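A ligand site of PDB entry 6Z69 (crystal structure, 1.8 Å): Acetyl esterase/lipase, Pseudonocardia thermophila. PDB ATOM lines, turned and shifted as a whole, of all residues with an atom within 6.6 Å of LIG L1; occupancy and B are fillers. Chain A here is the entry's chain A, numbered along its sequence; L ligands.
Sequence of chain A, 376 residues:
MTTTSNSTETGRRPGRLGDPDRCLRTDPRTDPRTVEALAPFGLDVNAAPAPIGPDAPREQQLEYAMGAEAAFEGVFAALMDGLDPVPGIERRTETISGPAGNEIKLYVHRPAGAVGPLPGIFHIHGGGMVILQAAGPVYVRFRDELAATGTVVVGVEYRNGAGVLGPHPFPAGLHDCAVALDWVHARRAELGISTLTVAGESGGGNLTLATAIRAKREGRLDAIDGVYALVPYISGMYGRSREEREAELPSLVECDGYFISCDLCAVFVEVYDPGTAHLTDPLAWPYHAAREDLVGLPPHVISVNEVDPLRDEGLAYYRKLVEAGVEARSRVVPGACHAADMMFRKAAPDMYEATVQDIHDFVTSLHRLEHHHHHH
N of Gly 128 lies within hydrogen-bond range of O1 of LG2 L2, at 2.8 Å. The backbone NH of Gly 203 is in hydrogen-bond range of an oxygen (O1) of LIG L1. A phosphorus (P1) of LIG L1 is covalently linked to the side-chain hydroxyl (OG) of Ser 202. N of Gly 128 lies within hydrogen-bond range of O1 of LIG L1, at 2.8 Å. The backbone NH of Gly 127 sits at hydrogen-bond distance from an oxygen (O1) of LIG L1 (2.8 Å).
OE2 of Glu 201 sits at hydrogen-bond distance from OH of Tyr 139 (2.6 Å). The side-chain hydroxyl (OG) of Ser 202 sits at hydrogen-bond distance from a ring nitrogen (NE2) of His 338 (3.0 Å). N of Gly 126 is in hydrogen-bond range of OE2 of Glu 201 (2.9 Å). The backbone carbonyl oxygen (O) of Ser 202 sits at hydrogen-bond distance from the backbone NH (N) of Tyr 233, 3.2 Å away. The backbone NH (N) of Ser 202 lies close to the backbone carbonyl oxygen (O) of Val 231 (3.1 Å). The side-chain hydroxyl (OH) of Tyr 139 sits at hydrogen-bond distance from the backbone NH (N) of Gly 126 (3.3 Å).
Residues that only touch LIG L1: Tyr 233 (2.8 Å), His 338 (3.2 Å), Glu 201 (3.5 Å), Tyr 139 (3.5 Å), Ala 339 (3.6 Å), Gly 126 (3.8 Å), Phe 76 (3.8 Å) and Met 343 (3.9 Å). Hydrophobic or aromatic side chains that line LIG L1: Phe 76, Tyr 233, His 338, Ala 339 and Met 343. 12 residues have an atom within 4 Å of LIG L1: Phe 76, Gly 126, Gly 127, Gly 128, Tyr 139, Glu 201, Ser 202, Gly 203, Tyr 233, His 338, Ala 339 and Met 343. The nearest printed residue that does not touch LIG L1 is Val 138 (4.05 Å).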
ATOM      1  N   PHE A  76      11.712  -5.375  30.280  1.00  0.00           N
ATOM      2  CA  PHE A  76      10.866  -4.850  29.172  1.00  0.00           C
ATOM      3  C   PHE A  76       9.439  -5.333  29.343  1.00  0.00           C
ATOM      4  O   PHE A  76       8.503  -4.505  29.171  1.00  0.00           O
ATOM      5  CB  PHE A  76      11.481  -5.213  27.825  1.00  0.00           C
ATOM      6  CG  PHE A  76      12.824  -4.560  27.613  1.00  0.00           C
ATOM      7  CD1 PHE A  76      13.135  -3.352  28.219  1.00  0.00           C
ATOM      8  CD2 PHE A  76      13.797  -5.194  26.882  1.00  0.00           C
ATOM      9  CE1 PHE A  76      14.358  -2.742  28.028  1.00  0.00           C
ATOM     10  CE2 PHE A  76      15.042  -4.610  26.728  1.00  0.00           C
ATOM     11  CZ  PHE A  76      15.310  -3.387  27.294  1.00  0.00           C
ATOM     12  N   HIS A 125      14.467  -4.422  15.261  1.00  0.00           N
ATOM     13  CA  HIS A 125      14.561  -4.253  16.725  1.00  0.00           C
ATOM     14  C   HIS A 125      16.023  -4.083  17.165  1.00  0.00           C
ATOM     15  O   HIS A 125      16.947  -4.603  16.480  1.00  0.00           O
ATOM     16  CB  HIS A 125      13.881  -5.411  17.458  1.00  0.00           C
ATOM     17  CG  HIS A 125      14.640  -6.696  17.333  1.00  0.00           C
ATOM     18  ND1 HIS A 125      15.687  -6.983  18.139  1.00  0.00           N
ATOM     19  CD2 HIS A 125      14.547  -7.704  16.445  1.00  0.00           C
ATOM     20  CE1 HIS A 125      16.209  -8.147  17.803  1.00  0.00           C
ATOM     21  NE2 HIS A 125      15.473  -8.651  16.815  1.00  0.00           N
ATOM     22  N   GLY A 126      16.201  -3.488  18.323  1.00  0.00           N
ATOM     23  CA  GLY A 126      17.496  -3.361  18.999  1.00  0.00           C
ATOM     24  C   GLY A 126      17.858  -4.553  19.884  1.00  0.00           C
ATOM     25  O   GLY A 126      17.145  -5.603  19.890  1.00  0.00           O
ATOM     26  N   GLY A 127      18.958  -4.402  20.588  1.00  0.00           N
ATOM     27  CA  GLY A 127      19.628  -5.481  21.346  1.00  0.00           C
ATOM     28  C   GLY A 127      21.026  -5.715  20.833  1.00  0.00           C
ATOM     29  O   GLY A 127      21.500  -6.860  20.899  1.00  0.00           O
ATOM     30  N   GLY A 128      21.697  -4.671  20.355  1.00  0.00           N
ATOM     31  CA  GLY A 128      23.144  -4.729  19.998  1.00  0.00           C
ATOM     32  C   GLY A 128      23.457  -5.753  18.927  1.00  0.00           C
ATOM     33  O   GLY A 128      24.628  -6.174  18.835  1.00  0.00           O
ATOM     34  N   MET A 129      22.468  -6.111  18.092  1.00  0.00           N
ATOM     35  CA  MET A 129      22.520  -7.168  17.041  1.00  0.00           C
ATOM     36  C   MET A 129      22.828  -8.541  17.641  1.00  0.00           C
ATOM     37  O   MET A 129      23.040  -9.502  16.848  1.00  0.00           O
ATOM     38  CB  MET A 129      23.544  -6.820  15.966  1.00  0.00           C
ATOM     39  CG  MET A 129      23.269  -5.474  15.318  1.00  0.00           C
ATOM     40  SD  MET A 129      24.060  -4.024  16.086  1.00  0.00           S
ATOM     41  CE  MET A 129      25.792  -4.385  15.813  1.00  0.00           C
ATOM     42  N   LEU A 132      17.636 -10.107  22.308  1.00  0.00           N
ATOM     43  CA  LEU A 132      16.237  -9.611  22.371  1.00  0.00           C
ATOM     44  C   LEU A 132      15.477 -10.097  21.124  1.00  0.00           C
ATOM     45  O   LEU A 132      16.104 -10.268  20.067  1.00  0.00           O
ATOM     46  CB  LEU A 132      16.170  -8.073  22.440  1.00  0.00           C
ATOM     47  CG  LEU A 132      16.885  -7.417  23.623  1.00  0.00           C
ATOM     48  CD1 LEU A 132      16.751  -5.876  23.543  1.00  0.00           C
ATOM     49  CD2 LEU A 132      16.415  -7.979  24.965  1.00  0.00           C
ATOM     50  N   VAL A 138       7.998  -5.032  24.267  1.00  0.00           N
ATOM     51  CA  VAL A 138       8.468  -3.657  23.954  1.00  0.00           C
ATOM     52  C   VAL A 138       8.321  -3.406  22.428  1.00  0.00           C
ATOM     53  O   VAL A 138       7.923  -2.303  22.023  1.00  0.00           O
ATOM     54  CB  VAL A 138       9.871  -3.365  24.520  1.00  0.00           C
ATOM     55  CG1 VAL A 138      11.006  -4.053  23.780  1.00  0.00           C
ATOM     56  CG2 VAL A 138      10.160  -1.889  24.575  1.00  0.00           C
ATOM     57  N   TYR A 139       8.638  -4.382  21.584  1.00  0.00           N
ATOM     58  CA  TYR A 139       8.644  -4.234  20.100  1.00  0.00           C
ATOM     59  C   TYR A 139       7.233  -4.448  19.574  1.00  0.00           C
ATOM     60  O   TYR A 139       6.798  -3.723  18.643  1.00  0.00           O
ATOM     61  CB  TYR A 139       9.725  -5.124  19.465  1.00  0.00           C
ATOM     62  CG  TYR A 139      11.099  -4.719  19.922  1.00  0.00           C
ATOM     63  CD1 TYR A 139      11.604  -3.469  19.615  1.00  0.00           C
ATOM     64  CD2 TYR A 139      11.837  -5.529  20.780  1.00  0.00           C
ATOM     65  CE1 TYR A 139      12.837  -3.048  20.066  1.00  0.00           C
ATOM     66  CE2 TYR A 139      13.106  -5.138  21.212  1.00  0.00           C
ATOM     67  CZ  TYR A 139      13.594  -3.883  20.874  1.00  0.00           C
ATOM     68  OH  TYR A 139      14.820  -3.465  21.318  1.00  0.00           O
ATOM     69  N   GLU A 201      15.946   1.137  16.318  1.00  0.00           N
ATOM     70  CA  GLU A 201      16.702   1.815  17.401  1.00  0.00           C
ATOM     71  C   GLU A 201      17.924   0.994  17.801  1.00  0.00           C
ATOM     72  O   GLU A 201      17.851  -0.274  17.841  1.00  0.00           O
ATOM     73  CB  GLU A 201      15.785   2.065  18.595  1.00  0.00           C
ATOM     74  CG  GLU A 201      15.788   1.001  19.673  1.00  0.00           C
ATOM     75  CD  GLU A 201      15.226  -0.368  19.346  1.00  0.00           C
ATOM     76  OE1 GLU A 201      14.542  -0.523  18.338  1.00  0.00           O
ATOM     77  OE2 GLU A 201      15.563  -1.288  20.103  1.00  0.00           O
ATOM     78  N   SER A 202      18.977   1.708  18.175  1.00  0.00           N
ATOM     79  CA  SER A 202      20.181   1.141  18.844  1.00  0.00           C
ATOM     80  C   SER A 202      20.774   0.129  17.883  1.00  0.00           C
ATOM     81  O   SER A 202      21.030   0.527  16.754  1.00  0.00           O
ATOM     82  CB  SER A 202      19.802   0.611  20.215  1.00  0.00           C
ATOM     83  OG  SER A 202      20.942   0.265  20.991  1.00  0.00           O
ATOM     84  N   GLY A 203      20.867  -1.153  18.252  1.00  0.00           N
ATOM     85  CA  GLY A 203      21.356  -2.183  17.313  1.00  0.00           C
ATOM     86  C   GLY A 203      20.501  -2.259  16.051  1.00  0.00           C
ATOM     87  O   GLY A 203      21.025  -2.584  15.000  1.00  0.00           O
ATOM     88  N   GLY A 204      19.217  -2.002  16.165  1.00  0.00           N
ATOM     89  CA  GLY A 204      18.267  -1.990  15.024  1.00  0.00           C
ATOM     90  C   GLY A 204      18.503  -0.760  14.161  1.00  0.00           C
ATOM     91  O   GLY A 204      18.232  -0.805  12.924  1.00  0.00           O
ATOM     92  N   VAL A 231      18.561   6.452  18.051  1.00  0.00           N
ATOM     93  CA  VAL A 231      19.667   6.173  19.021  1.00  0.00           C
ATOM     94  C   VAL A 231      20.589   5.105  18.431  1.00  0.00           C
ATOM     95  O   VAL A 231      20.825   4.060  19.026  1.00  0.00           O
ATOM     96  CB  VAL A 231      19.076   5.799  20.393  1.00  0.00           C
ATOM     97  CG1 VAL A 231      18.339   6.992  20.987  1.00  0.00           C
ATOM     98  CG2 VAL A 231      18.131   4.591  20.355  1.00  0.00           C
ATOM     99  N   TYR A 233      23.407   2.570  17.329  1.00  0.00           N
ATOM    100  CA  TYR A 233      24.550   1.867  17.968  1.00  0.00           C
ATOM    101  C   TYR A 233      25.548   1.506  16.877  1.00  0.00           C
ATOM    102  O   TYR A 233      25.447   0.392  16.343  1.00  0.00           O
ATOM    103  CB  TYR A 233      23.979   0.670  18.720  1.00  0.00           C
ATOM    104  CG  TYR A 233      24.954  -0.309  19.318  1.00  0.00           C
ATOM    105  CD1 TYR A 233      25.672  -0.025  20.463  1.00  0.00           C
ATOM    106  CD2 TYR A 233      25.058  -1.590  18.781  1.00  0.00           C
ATOM    107  CE1 TYR A 233      26.532  -0.951  21.023  1.00  0.00           C
ATOM    108  CE2 TYR A 233      25.911  -2.529  19.340  1.00  0.00           C
ATOM    109  CZ  TYR A 233      26.622  -2.232  20.484  1.00  0.00           C
ATOM    110  OH  TYR A 233      27.434  -3.193  21.020  1.00  0.00           O
ATOM    111  N   TYR A 238      33.316   1.021  21.888  1.00  0.00           N
ATOM    112  CA  TYR A 238      32.968   1.024  23.323  1.00  0.00           C
ATOM    113  C   TYR A 238      34.166   0.503  24.125  1.00  0.00           C
ATOM    114  O   TYR A 238      34.262   0.914  25.286  1.00  0.00           O
ATOM    115  CB  TYR A 238      31.635   0.265  23.525  1.00  0.00           C
ATOM    116  CG  TYR A 238      30.656   0.622  22.431  1.00  0.00           C
ATOM    117  CD1 TYR A 238      30.204   1.921  22.274  1.00  0.00           C
ATOM    118  CD2 TYR A 238      30.307  -0.297  21.458  1.00  0.00           C
ATOM    119  CE1 TYR A 238      29.407   2.284  21.208  1.00  0.00           C
ATOM    120  CE2 TYR A 238      29.504   0.046  20.380  1.00  0.00           C
ATOM    121  CZ  TYR A 238      29.047   1.345  20.257  1.00  0.00           C
ATOM    122  OH  TYR A 238      28.342   1.694  19.138  1.00  0.00           O
ATOM    123  N   PHE A 259      21.948   3.659  31.737  1.00  0.00           N
ATOM    124  CA  PHE A 259      21.150   2.529  31.175  1.00  0.00           C
ATOM    125  C   PHE A 259      22.068   1.505  30.475  1.00  0.00           C
ATOM    126  O   PHE A 259      21.976   0.259  30.734  1.00  0.00           O
ATOM    127  CB  PHE A 259      20.039   3.013  30.233  1.00  0.00           C
ATOM    128  CG  PHE A 259      19.129   1.877  29.832  1.00  0.00           C
ATOM    129  CD1 PHE A 259      18.288   1.301  30.763  1.00  0.00           C
ATOM    130  CD2 PHE A 259      19.169   1.352  28.555  1.00  0.00           C
ATOM    131  CE1 PHE A 259      17.487   0.216  30.422  1.00  0.00           C
ATOM    132  CE2 PHE A 259      18.389   0.253  28.217  1.00  0.00           C
ATOM    133  CZ  PHE A 259      17.557  -0.303  29.142  1.00  0.00           C
ATOM    134  N   ILE A 260      22.921   1.970  29.564  1.00  0.00           N
ATOM    135  CA  ILE A 260      23.919   1.098  28.867  1.00  0.00           C
ATOM    136  C   ILE A 260      25.340   1.504  29.230  1.00  0.00           C
ATOM    137  O   ILE A 260      25.587   2.716  29.549  1.00  0.00           O
ATOM    138  CB  ILE A 260      23.668   1.060  27.347  1.00  0.00           C
ATOM    139  CG1 ILE A 260      23.759   2.437  26.697  1.00  0.00           C
ATOM    140  CG2 ILE A 260      22.339   0.338  27.008  1.00  0.00           C
ATOM    141  CD1 ILE A 260      23.939   2.362  25.196  1.00  0.00           C
ATOM    142  N   CYS A 265      28.928  -3.268  26.236  1.00  0.00           N
ATOM    143  CA  CYS A 265      28.827  -3.110  24.762  1.00  0.00           C
ATOM    144  C   CYS A 265      30.118  -3.657  24.151  1.00  0.00           C
ATOM    145  O   CYS A 265      30.057  -4.319  23.112  1.00  0.00           O
ATOM    146  CB  CYS A 265      28.577  -1.672  24.356  1.00  0.00           C
ATOM    147  SG  CYS A 265      26.927  -1.083  24.830  1.00  0.00           S
ATOM    148  N   PHE A 268      29.788  -7.113  23.657  1.00  0.00           N
ATOM    149  CA  PHE A 268      28.751  -7.444  22.642  1.00  0.00           C
ATOM    150  C   PHE A 268      29.332  -7.187  21.240  1.00  0.00           C
ATOM    151  O   PHE A 268      28.906  -7.836  20.267  1.00  0.00           O
ATOM    152  CB  PHE A 268      27.467  -6.648  22.909  1.00  0.00           C
ATOM    153  CG  PHE A 268      26.586  -7.128  24.038  1.00  0.00           C
ATOM    154  CD1 PHE A 268      26.879  -8.286  24.745  1.00  0.00           C
ATOM    155  CD2 PHE A 268      25.485  -6.383  24.409  1.00  0.00           C
ATOM    156  CE1 PHE A 268      26.057  -8.696  25.775  1.00  0.00           C
ATOM    157  CE2 PHE A 268      24.655  -6.805  25.439  1.00  0.00           C
ATOM    158  CZ  PHE A 268      24.966  -7.957  26.125  1.00  0.00           C
ATOM    159  N   LEU A 310      25.471   6.971  23.276  1.00  0.00           N
ATOM    160  CA  LEU A 310      25.520   6.887  21.788  1.00  0.00           C
ATOM    161  C   LEU A 310      25.185   8.232  21.109  1.00  0.00           C
ATOM    162  O   LEU A 310      25.217   8.268  19.874  1.00  0.00           O
ATOM    163  CB  LEU A 310      24.578   5.778  21.313  1.00  0.00           C
ATOM    164  CG  LEU A 310      24.778   4.428  21.992  1.00  0.00           C
ATOM    165  CD1 LEU A 310      23.774   3.429  21.486  1.00  0.00           C
ATOM    166  CD2 LEU A 310      26.210   3.893  21.811  1.00  0.00           C
ATOM    167  N   HIS A 338      19.241   6.526  26.767  1.00  0.00           N
ATOM    168  CA  HIS A 338      19.142   5.600  25.609  1.00  0.00           C
ATOM    169  C   HIS A 338      17.749   4.943  25.541  1.00  0.00           C
ATOM    170  O   HIS A 338      17.324   4.333  26.546  1.00  0.00           O
ATOM    171  CB  HIS A 338      20.209   4.539  25.706  1.00  0.00           C
ATOM    172  CG  HIS A 338      20.160   3.642  24.514  1.00  0.00           C
ATOM    173  ND1 HIS A 338      20.596   4.083  23.273  1.00  0.00           N
ATOM    174  CD2 HIS A 338      19.541   2.452  24.324  1.00  0.00           C
ATOM    175  CE1 HIS A 338      20.334   3.126  22.387  1.00  0.00           C
ATOM    176  NE2 HIS A 338      19.713   2.107  22.998  1.00  0.00           N
ATOM    177  N   ALA A 339      17.063   5.086  24.397  1.00  0.00           N
ATOM    178  CA  ALA A 339      15.782   4.443  24.058  1.00  0.00           C
ATOM    179  C   ALA A 339      14.671   4.827  25.036  1.00  0.00           C
ATOM    180  O   ALA A 339      13.635   4.124  25.048  1.00  0.00           O
ATOM    181  CB  ALA A 339      15.964   2.939  23.992  1.00  0.00           C
ATOM    182  N   MET A 342      11.190   4.888  23.771  1.00  0.00           N
ATOM    183  CA  MET A 342      10.513   3.632  23.388  1.00  0.00           C
ATOM    184  C   MET A 342      10.282   2.729  24.593  1.00  0.00           C
ATOM    185  O   MET A 342       9.467   1.817  24.459  1.00  0.00           O
ATOM    186  CB  MET A 342      11.323   2.901  22.312  1.00  0.00           C
ATOM    187  CG  MET A 342      11.231   3.660  20.992  1.00  0.00           C
ATOM    188  SD  MET A 342      12.457   3.093  19.745  1.00  0.00           S
ATOM    189  CE  MET A 342      12.303   1.364  20.215  1.00  0.00           C
ATOM    190  N   MET A 343      10.942   2.984  25.737  1.00  0.00           N
ATOM    191  CA  MET A 343      10.772   2.151  26.949  1.00  0.00           C
ATOM    192  C   MET A 343       9.651   2.675  27.844  1.00  0.00           C
ATOM    193  O   MET A 343       8.972   1.832  28.429  1.00  0.00           O
ATOM    194  CB  MET A 343      12.064   2.041  27.760  1.00  0.00           C
ATOM    195  CG  MET A 343      13.153   1.326  26.974  1.00  0.00           C
ATOM    196  SD  MET A 343      14.557   0.915  28.010  1.00  0.00           S
ATOM    197  CE  MET A 343      15.230   2.551  28.320  1.00  0.00           C
HETATM  198  C1  LIG L   1      20.018  -1.023  23.237  1.00  0.00           C
HETATM  199  C2  LIG L   1      18.534  -1.094  23.020  1.00  0.00           C
HETATM  200  C3  LIG L   1      17.803  -1.338  24.322  1.00  0.00           C
HETATM  201  C4  LIG L   1      16.368  -1.755  24.009  1.00  0.00           C
HETATM  202  C5  LIG L   1      15.497  -0.599  23.528  1.00  0.00           C
HETATM  203  C6  LIG L   1      14.018  -0.900  23.861  1.00  0.00           C
HETATM  204  P1  LIG L   1      20.984  -1.039  21.756  1.00  0.00           P
HETATM  205  O1  LIG L   1      20.648  -2.155  20.820  1.00  0.00           O
HETATM  206  O2  LIG L   1      22.376  -1.188  22.550  1.00  0.00           O
HETATM  207  C7  LIG L   1      23.555  -1.110  21.944  1.00  0.00           C
HETATM  208  C1  LG2 L   2      21.682  -3.157  28.452  1.00  0.00           C
HETATM  209  C2  LG2 L   2      22.829  -2.678  29.107  1.00  0.00           C
HETATM  210  C3  LG2 L   2      24.081  -2.572  28.382  1.00  0.00           C
HETATM  211  C4  LG2 L   2      21.993  -4.274  24.403  1.00  0.00           C
HETATM  212  C5  LG2 L   2      20.663  -4.424  25.049  1.00  0.00           C
HETATM  213  C6  LG2 L   2      20.602  -4.041  26.365  1.00  0.00           C
HETATM  214  O1  LG2 L   2      22.142  -4.605  23.091  1.00  0.00           O
HETATM  215  O2  LG2 L   2      23.078  -3.762  25.056  1.00  0.00           O
HETATM  216  C7  LG2 L   2      19.254  -4.174  27.050  1.00  0.00           C
HETATM  217  C8  LG2 L   2      21.722  -3.564  27.064  1.00  0.00           C
HETATM  218  C9  LG2 L   2      23.007  -3.407  26.383  1.00  0.00           C
HETATM  219  C10 LG2 L   2      24.117  -2.933  26.987  1.00  0.00           C
HETATM  220  O3  LG2 L   2      25.195  -2.083  29.080  1.00  0.00           O
